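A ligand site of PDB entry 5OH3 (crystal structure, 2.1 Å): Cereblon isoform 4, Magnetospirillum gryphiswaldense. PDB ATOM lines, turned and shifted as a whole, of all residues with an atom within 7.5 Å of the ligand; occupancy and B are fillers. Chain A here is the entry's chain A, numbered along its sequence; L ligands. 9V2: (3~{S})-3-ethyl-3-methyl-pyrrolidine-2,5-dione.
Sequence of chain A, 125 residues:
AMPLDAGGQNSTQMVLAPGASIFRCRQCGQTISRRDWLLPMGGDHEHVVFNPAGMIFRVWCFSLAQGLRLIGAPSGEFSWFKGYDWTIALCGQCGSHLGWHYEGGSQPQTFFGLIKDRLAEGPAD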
ATOM      1  N   VAL A  49     -20.948  -3.902 -10.491  1.00  0.00           N
ATOM      2  CA  VAL A  49     -21.938  -3.705 -11.546  1.00  0.00           C
ATOM      3  C   VAL A  49     -21.905  -4.843 -12.567  1.00  0.00           C
ATOM      4  O   VAL A  49     -20.927  -5.608 -12.654  1.00  0.00           O
ATOM      5  CB  VAL A  49     -21.684  -2.360 -12.273  1.00  0.00           C
ATOM      6  CG1 VAL A  49     -21.900  -1.189 -11.328  1.00  0.00           C
ATOM      7  CG2 VAL A  49     -20.268  -2.302 -12.832  1.00  0.00           C
ATOM      8  N   PHE A  50     -22.987  -4.950 -13.334  1.00  0.00           N
ATOM      9  CA  PHE A  50     -23.115  -5.931 -14.390  1.00  0.00           C
ATOM     10  C   PHE A  50     -23.376  -5.268 -15.719  1.00  0.00           C
ATOM     11  O   PHE A  50     -24.120  -4.303 -15.802  1.00  0.00           O
ATOM     12  CB  PHE A  50     -24.311  -6.845 -14.132  1.00  0.00           C
ATOM     13  CG  PHE A  50     -24.142  -7.784 -12.981  1.00  0.00           C
ATOM     14  CD1 PHE A  50     -23.538  -9.024 -13.160  1.00  0.00           C
ATOM     15  CD2 PHE A  50     -24.639  -7.461 -11.719  1.00  0.00           C
ATOM     16  CE1 PHE A  50     -23.375  -9.906 -12.101  1.00  0.00           C
ATOM     17  CE2 PHE A  50     -24.490  -8.342 -10.656  1.00  0.00           C
ATOM     18  CZ  PHE A  50     -23.866  -9.574 -10.846  1.00  0.00           C
ATOM     19  N   ASN A  51     -22.827  -5.866 -16.773  1.00  0.00           N
ATOM     20  CA  ASN A  51     -23.131  -5.447 -18.138  1.00  0.00           C
ATOM     21  C   ASN A  51     -24.259  -6.298 -18.740  1.00  0.00           C
ATOM     22  O   ASN A  51     -24.726  -7.215 -18.084  1.00  0.00           O
ATOM     23  CB  ASN A  51     -21.855  -5.442 -19.003  1.00  0.00           C
ATOM     24  CG  ASN A  51     -21.321  -6.827 -19.296  1.00  0.00           C
ATOM     25  OD1 ASN A  51     -21.962  -7.868 -19.049  1.00  0.00           O
ATOM     26  ND2 ASN A  51     -20.151  -6.853 -19.890  1.00  0.00           N
ATOM     27  N   PRO A  52     -24.733  -5.953 -19.951  1.00  0.00           N
ATOM     28  CA  PRO A  52     -25.841  -6.742 -20.517  1.00  0.00           C
ATOM     29  C   PRO A  52     -25.496  -8.199 -20.859  1.00  0.00           C
ATOM     30  O   PRO A  52     -26.394  -8.996 -21.059  1.00  0.00           O
ATOM     31  CB  PRO A  52     -26.217  -5.954 -21.788  1.00  0.00           C
ATOM     32  CG  PRO A  52     -25.744  -4.557 -21.527  1.00  0.00           C
ATOM     33  CD  PRO A  52     -24.504  -4.704 -20.698  1.00  0.00           C
ATOM     34  N   ALA A  53     -24.214  -8.536 -20.940  1.00  0.00           N
ATOM     35  CA  ALA A  53     -23.798  -9.914 -21.138  1.00  0.00           C
ATOM     36  C   ALA A  53     -23.675 -10.656 -19.808  1.00  0.00           C
ATOM     37  O   ALA A  53     -23.272 -11.830 -19.773  1.00  0.00           O
ATOM     38  CB  ALA A  53     -22.484  -9.961 -21.905  1.00  0.00           C
ATOM     39  N   MET A  55     -21.712 -10.087 -17.247  1.00  0.00           N
ATOM     40  CA  MET A  55     -20.408 -10.068 -16.568  1.00  0.00           C
ATOM     41  C   MET A  55     -20.452  -9.080 -15.423  1.00  0.00           C
ATOM     42  O   MET A  55     -20.982  -7.969 -15.576  1.00  0.00           O
ATOM     43  CB  MET A  55     -19.310  -9.670 -17.522  1.00  0.00           C
ATOM     44  CG  MET A  55     -19.262 -10.497 -18.792  1.00  0.00           C
ATOM     45  SD  MET A  55     -17.906  -9.966 -19.838  1.00  0.00           S
ATOM     46  CE  MET A  55     -18.740  -9.345 -21.311  1.00  0.00           C
ATOM     47  N   PHE A  57     -18.478  -6.734 -12.754  1.00  0.00           N
ATOM     48  CA  PHE A  57     -17.223  -5.988 -12.703  1.00  0.00           C
ATOM     49  C   PHE A  57     -17.193  -5.276 -11.373  1.00  0.00           C
ATOM     50  O   PHE A  57     -18.193  -4.702 -10.943  1.00  0.00           O
ATOM     51  CB  PHE A  57     -17.137  -4.945 -13.823  1.00  0.00           C
ATOM     52  CG  PHE A  57     -17.173  -5.515 -15.206  1.00  0.00           C
ATOM     53  CD1 PHE A  57     -16.028  -5.986 -15.814  1.00  0.00           C
ATOM     54  CD2 PHE A  57     -18.350  -5.517 -15.941  1.00  0.00           C
ATOM     55  CE1 PHE A  57     -16.068  -6.495 -17.116  1.00  0.00           C
ATOM     56  CE2 PHE A  57     -18.382  -6.009 -17.227  1.00  0.00           C
ATOM     57  CZ  PHE A  57     -17.242  -6.503 -17.815  1.00  0.00           C
ATOM     58  N   SER A  75     -20.960   6.963 -25.488  1.00  0.00           N
ATOM     59  CA  SER A  75     -22.308   6.432 -25.567  1.00  0.00           C
ATOM     60  C   SER A  75     -22.957   6.485 -24.173  1.00  0.00           C
ATOM     61  O   SER A  75     -22.301   6.161 -23.182  1.00  0.00           O
ATOM     62  CB  SER A  75     -22.269   4.978 -26.053  1.00  0.00           C
ATOM     63  OG  SER A  75     -23.580   4.412 -26.000  1.00  0.00           O
ATOM     64  N   GLY A  76     -24.210   6.901 -24.106  1.00  0.00           N
ATOM     65  CA  GLY A  76     -25.003   6.841 -22.888  1.00  0.00           C
ATOM     66  C   GLY A  76     -25.682   5.486 -22.633  1.00  0.00           C
ATOM     67  O   GLY A  76     -26.172   5.248 -21.544  1.00  0.00           O
ATOM     68  N   GLU A  77     -25.704   4.600 -23.626  1.00  0.00           N
ATOM     69  CA  GLU A  77     -26.448   3.327 -23.493  1.00  0.00           C
ATOM     70  C   GLU A  77     -25.946   2.444 -22.351  1.00  0.00           C
ATOM     71  O   GLU A  77     -24.757   2.168 -22.252  1.00  0.00           O
ATOM     72  CB  GLU A  77     -26.376   2.553 -24.805  1.00  0.00           C
ATOM     73  CG  GLU A  77     -27.244   3.174 -25.886  1.00  0.00           C
ATOM     74  CD  GLU A  77     -26.898   2.703 -27.283  1.00  0.00           C
ATOM     75  OE1 GLU A  77     -25.995   1.862 -27.461  1.00  0.00           O
ATOM     76  OE2 GLU A  77     -27.572   3.178 -28.232  1.00  0.00           O
ATOM     77  N   PHE A  78     -26.872   2.057 -21.474  1.00  0.00           N
ATOM     78  CA  PHE A  78     -26.602   1.174 -20.334  1.00  0.00           C
ATOM     79  C   PHE A  78     -25.634   1.764 -19.296  1.00  0.00           C
ATOM     80  O   PHE A  78     -25.062   1.010 -18.486  1.00  0.00           O
ATOM     81  CB  PHE A  78     -26.028  -0.182 -20.797  1.00  0.00           C
ATOM     82  CG  PHE A  78     -26.889  -0.931 -21.784  1.00  0.00           C
ATOM     83  CD1 PHE A  78     -28.118  -1.438 -21.398  1.00  0.00           C
ATOM     84  CD2 PHE A  78     -26.433  -1.182 -23.065  1.00  0.00           C
ATOM     85  CE1 PHE A  78     -28.915  -2.151 -22.292  1.00  0.00           C
ATOM     86  CE2 PHE A  78     -27.216  -1.896 -23.963  1.00  0.00           C
ATOM     87  CZ  PHE A  78     -28.451  -2.382 -23.579  1.00  0.00           C
ATOM     88  N   SER A  79     -25.425   3.082 -19.297  1.00  0.00           N
ATOM     89  CA  SER A  79     -24.432   3.676 -18.393  1.00  0.00           C
ATOM     90  C   SER A  79     -24.759   3.366 -16.945  1.00  0.00           C
ATOM     91  O   SER A  79     -25.894   3.544 -16.518  1.00  0.00           O
ATOM     92  CB  SER A  79     -24.338   5.199 -18.537  1.00  0.00           C
ATOM     93  OG  SER A  79     -23.261   5.687 -17.708  1.00  0.00           O
ATOM     94  N   TRP A  80     -23.752   2.926 -16.212  1.00  0.00           N
ATOM     95  CA  TRP A  80     -23.897   2.649 -14.789  1.00  0.00           C
ATOM     96  C   TRP A  80     -23.967   3.893 -13.953  1.00  0.00           C
ATOM     97  O   TRP A  80     -24.303   3.812 -12.795  1.00  0.00           O
ATOM     98  CB  TRP A  80     -22.732   1.795 -14.287  1.00  0.00           C
ATOM     99  CG  TRP A  80     -22.719   0.418 -14.841  1.00  0.00           C
ATOM    100  CD1 TRP A  80     -23.777  -0.450 -14.927  1.00  0.00           C
ATOM    101  CD2 TRP A  80     -21.593  -0.278 -15.368  1.00  0.00           C
ATOM    102  NE1 TRP A  80     -23.371  -1.638 -15.496  1.00  0.00           N
ATOM    103  CE2 TRP A  80     -22.033  -1.558 -15.765  1.00  0.00           C
ATOM    104  CE3 TRP A  80     -20.242   0.066 -15.559  1.00  0.00           C
ATOM    105  CZ2 TRP A  80     -21.186  -2.494 -16.343  1.00  0.00           C
ATOM    106  CZ3 TRP A  80     -19.401  -0.852 -16.116  1.00  0.00           C
ATOM    107  CH2 TRP A  80     -19.876  -2.126 -16.510  1.00  0.00           C
ATOM    108  N   PHE A  81     -23.592   5.039 -14.522  1.00  0.00           N
ATOM    109  CA  PHE A  81     -23.507   6.277 -13.763  1.00  0.00           C
ATOM    110  C   PHE A  81     -24.353   7.317 -14.445  1.00  0.00           C
ATOM    111  O   PHE A  81     -24.070   7.711 -15.571  1.00  0.00           O
ATOM    112  CB  PHE A  81     -22.062   6.745 -13.656  1.00  0.00           C
ATOM    113  CG  PHE A  81     -21.160   5.759 -12.987  1.00  0.00           C
ATOM    114  CD1 PHE A  81     -21.025   5.745 -11.591  1.00  0.00           C
ATOM    115  CD2 PHE A  81     -20.412   4.886 -13.740  1.00  0.00           C
ATOM    116  CE1 PHE A  81     -20.175   4.847 -10.978  1.00  0.00           C
ATOM    117  CE2 PHE A  81     -19.562   3.989 -13.128  1.00  0.00           C
ATOM    118  CZ  PHE A  81     -19.439   3.980 -11.750  1.00  0.00           C
ATOM    119  N   TYR A  84     -23.778  10.250 -17.278  1.00  0.00           N
ATOM    120  CA  TYR A  84     -22.490  10.075 -17.906  1.00  0.00           C
ATOM    121  C   TYR A  84     -22.594   9.140 -19.094  1.00  0.00           C
ATOM    122  O   TYR A  84     -23.290   8.125 -19.036  1.00  0.00           O
ATOM    123  CB  TYR A  84     -21.472   9.514 -16.923  1.00  0.00           C
ATOM    124  CG  TYR A  84     -21.133  10.436 -15.789  1.00  0.00           C
ATOM    125  CD1 TYR A  84     -20.089  11.355 -15.891  1.00  0.00           C
ATOM    126  CD2 TYR A  84     -21.833  10.383 -14.589  1.00  0.00           C
ATOM    127  CE1 TYR A  84     -19.771  12.201 -14.841  1.00  0.00           C
ATOM    128  CE2 TYR A  84     -21.521  11.218 -13.532  1.00  0.00           C
ATOM    129  CZ  TYR A  84     -20.492  12.132 -13.653  1.00  0.00           C
ATOM    130  OH  TYR A  84     -20.224  12.953 -12.586  1.00  0.00           O
ATOM    131  N   ASP A  85     -21.818   9.483 -20.124  1.00  0.00           N
ATOM    132  CA  ASP A  85     -21.578   8.669 -21.290  1.00  0.00           C
ATOM    133  C   ASP A  85     -20.197   8.019 -21.184  1.00  0.00           C
ATOM    134  O   ASP A  85     -19.279   8.615 -20.618  1.00  0.00           O
ATOM    135  CB  ASP A  85     -21.606   9.581 -22.501  1.00  0.00           C
ATOM    136  CG  ASP A  85     -22.883  10.414 -22.518  1.00  0.00           C
ATOM    137  OD1 ASP A  85     -23.976   9.834 -22.357  1.00  0.00           O
ATOM    138  OD2 ASP A  85     -22.784  11.668 -22.582  1.00  0.00           O
ATOM    139  N   TRP A  86     -20.076   6.816 -21.727  1.00  0.00           N
ATOM    140  CA  TRP A  86     -18.880   6.026 -21.559  1.00  0.00           C
ATOM    141  C   TRP A  86     -18.174   5.818 -22.873  1.00  0.00           C
ATOM    142  O   TRP A  86     -18.803   5.800 -23.947  1.00  0.00           O
ATOM    143  CB  TRP A  86     -19.187   4.659 -20.896  1.00  0.00           C
ATOM    144  CG  TRP A  86     -20.231   3.857 -21.587  1.00  0.00           C
ATOM    145  CD1 TRP A  86     -21.546   3.830 -21.291  1.00  0.00           C
ATOM    146  CD2 TRP A  86     -20.055   2.976 -22.710  1.00  0.00           C
ATOM    147  NE1 TRP A  86     -22.217   3.011 -22.168  1.00  0.00           N
ATOM    148  CE2 TRP A  86     -21.323   2.459 -23.042  1.00  0.00           C
ATOM    149  CE3 TRP A  86     -18.947   2.563 -23.461  1.00  0.00           C
ATOM    150  CZ2 TRP A  86     -21.523   1.562 -24.098  1.00  0.00           C
ATOM    151  CZ3 TRP A  86     -19.143   1.664 -24.504  1.00  0.00           C
ATOM    152  CH2 TRP A  86     -20.435   1.166 -24.802  1.00  0.00           C
ATOM    153  N   THR A  87     -16.852   5.675 -22.785  1.00  0.00           N
ATOM    154  CA  THR A  87     -16.037   5.137 -23.873  1.00  0.00           C
ATOM    155  C   THR A  87     -15.154   4.072 -23.274  1.00  0.00           C
ATOM    156  O   THR A  87     -14.703   4.195 -22.143  1.00  0.00           O
ATOM    157  CB  THR A  87     -15.120   6.187 -24.504  1.00  0.00           C
ATOM    158  OG1 THR A  87     -14.222   6.682 -23.510  1.00  0.00           O
ATOM    159  CG2 THR A  87     -15.901   7.321 -25.067  1.00  0.00           C
ATOM    160  N   ILE A  88     -14.927   3.002 -24.015  1.00  0.00           N
ATOM    161  CA  ILE A  88     -14.068   1.907 -23.601  1.00  0.00           C
ATOM    162  C   ILE A  88     -12.634   2.391 -23.444  1.00  0.00           C
ATOM    163  O   ILE A  88     -12.109   3.102 -24.307  1.00  0.00           O
ATOM    164  CB  ILE A  88     -14.145   0.760 -24.637  1.00  0.00           C
ATOM    165  CG1 ILE A  88     -15.509   0.058 -24.506  1.00  0.00           C
ATOM    166  CG2 ILE A  88     -13.016  -0.250 -24.426  1.00  0.00           C
ATOM    167  CD1 ILE A  88     -15.874  -0.810 -25.696  1.00  0.00           C
ATOM    168  N   HIS A  97      -8.485  -4.686 -21.824  1.00  0.00           N
ATOM    169  CA  HIS A  97      -9.627  -3.848 -21.481  1.00  0.00           C
ATOM    170  C   HIS A  97      -9.621  -3.535 -19.991  1.00  0.00           C
ATOM    171  O   HIS A  97      -9.869  -4.423 -19.168  1.00  0.00           O
ATOM    172  CB  HIS A  97     -10.932  -4.525 -21.864  1.00  0.00           C
ATOM    173  CG  HIS A  97     -12.138  -3.735 -21.467  1.00  0.00           C
ATOM    174  ND1 HIS A  97     -13.311  -4.306 -21.065  1.00  0.00           N
ATOM    175  CD2 HIS A  97     -12.317  -2.392 -21.382  1.00  0.00           C
ATOM    176  CE1 HIS A  97     -14.184  -3.365 -20.764  1.00  0.00           C
ATOM    177  NE2 HIS A  97     -13.604  -2.199 -20.946  1.00  0.00           N
ATOM    178  N   GLY A  99     -11.194  -0.687 -18.423  1.00  0.00           N
ATOM    179  CA  GLY A  99     -12.394  -0.051 -17.894  1.00  0.00           C
ATOM    180  C   GLY A  99     -13.032   0.898 -18.901  1.00  0.00           C
ATOM    181  O   GLY A  99     -13.095   0.601 -20.080  1.00  0.00           O
ATOM    182  N   TRP A 100     -13.535   1.999 -18.390  1.00  0.00           N
ATOM    183  CA  TRP A 100     -14.250   3.001 -19.185  1.00  0.00           C
ATOM    184  C   TRP A 100     -13.882   4.395 -18.707  1.00  0.00           C
ATOM    185  O   TRP A 100     -13.602   4.611 -17.517  1.00  0.00           O
ATOM    186  CB  TRP A 100     -15.766   2.769 -19.067  1.00  0.00           C
ATOM    187  CG  TRP A 100     -16.198   1.379 -19.488  1.00  0.00           C
ATOM    188  CD1 TRP A 100     -16.643   1.001 -20.708  1.00  0.00           C
ATOM    189  CD2 TRP A 100     -16.188   0.200 -18.676  1.00  0.00           C
ATOM    190  NE1 TRP A 100     -16.916  -0.324 -20.720  1.00  0.00           N
ATOM    191  CE2 TRP A 100     -16.650  -0.840 -19.484  1.00  0.00           C
ATOM    192  CE3 TRP A 100     -15.843  -0.068 -17.338  1.00  0.00           C
ATOM    193  CZ2 TRP A 100     -16.778  -2.161 -19.005  1.00  0.00           C
ATOM    194  CZ3 TRP A 100     -15.956  -1.359 -16.873  1.00  0.00           C
ATOM    195  CH2 TRP A 100     -16.415  -2.387 -17.701  1.00  0.00           C
ATOM    196  N   TYR A 102     -15.634   8.087 -18.403  1.00  0.00           N
ATOM    197  CA  TYR A 102     -16.951   8.684 -18.305  1.00  0.00           C
ATOM    198  C   TYR A 102     -16.866  10.200 -18.524  1.00  0.00           C
ATOM    199  O   TYR A 102     -15.945  10.849 -18.044  1.00  0.00           O
ATOM    200  CB  TYR A 102     -17.605   8.344 -16.958  1.00  0.00           C
ATOM    201  CG  TYR A 102     -17.991   6.906 -16.900  1.00  0.00           C
ATOM    202  CD1 TYR A 102     -19.236   6.453 -17.352  1.00  0.00           C
ATOM    203  CD2 TYR A 102     -17.094   5.956 -16.401  1.00  0.00           C
ATOM    204  CE1 TYR A 102     -19.582   5.111 -17.302  1.00  0.00           C
ATOM    205  CE2 TYR A 102     -17.421   4.619 -16.340  1.00  0.00           C
ATOM    206  CZ  TYR A 102     -18.649   4.184 -16.794  1.00  0.00           C
ATOM    207  OH  TYR A 102     -18.949   2.844 -16.741  1.00  0.00           O
HETATM  208  O1  9V2 L   1     -22.976  -2.015 -19.052  1.00  0.00           O
HETATM  209  C4  9V2 L   1     -22.294  -1.009 -19.176  1.00  0.00           C
HETATM  210  N   9V2 L   1     -22.489   0.150 -18.516  1.00  0.00           N
HETATM  211  C1  9V2 L   1     -21.103  -0.899 -20.093  1.00  0.00           C
HETATM  212  C3  9V2 L   1     -21.552  -0.617 -21.534  1.00  0.00           C
HETATM  213  C7  9V2 L   1     -22.461  -1.670 -22.141  1.00  0.00           C
HETATM  214  C5  9V2 L   1     -20.249  -2.148 -20.091  1.00  0.00           C
HETATM  215  C2  9V2 L   1     -20.415   0.337 -19.484  1.00  0.00           C
HETATM  216  C6  9V2 L   1     -21.465   0.895 -18.534  1.00  0.00           C
HETATM  217  O2  9V2 L   1     -21.347   1.926 -17.870  1.00  0.00           O
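The indole nitrogen (NE1) of Trp 80 sits at hydrogen-bond distance from the backbone carbonyl oxygen (O) of Phe 50, 2.8 Å away.
O of Glu 77 is in hydrogen-bond range of NE1 of Trp 86, 2.7 Å away.
N of Trp 86 lies within hydrogen-bond range of O of Ser 75 (2.7 Å).
The backbone NH of Ala 53 lies within hydrogen-bond range of the side-chain amide oxygen of Asn 51, at 3.0 Å.
N of Met 55 lies within hydrogen-bond range of OD1 of Asn 51, 2.9 Å away.
OG of Ser 79 lies within hydrogen-bond range of O of Phe 81 (3.1 Å).
The side-chain hydroxyl (OG) of Ser 79 lies within hydrogen-bond range of the backbone carbonyl oxygen (O) of Tyr 84, 2.8 Å away.
A nitrogen (N) of the ligand is in hydrogen-bond range of the backbone carbonyl oxygen of Phe 78 (2.7 Å).
The side-chain hydroxyl (OH) of Tyr 102 sits at hydrogen-bond distance from an oxygen (O2) of the ligand (2.8 Å).
The backbone NH (N) of Trp 80 lies within hydrogen-bond range of an oxygen (O2) of the ligand (3.1 Å).
Asn 51 touches the ligand.
Pro 52 touches the ligand.
Ser 79 touches the ligand.
Trp 86 touches the ligand.
Trp 100 touches the ligand (CZ2 to C5, 3.6 Å).
Hydrophobic or aromatic side chains that line the ligand: Pro 52, Phe 78, Trp 80, Trp 86, Trp 100 and Tyr 102.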
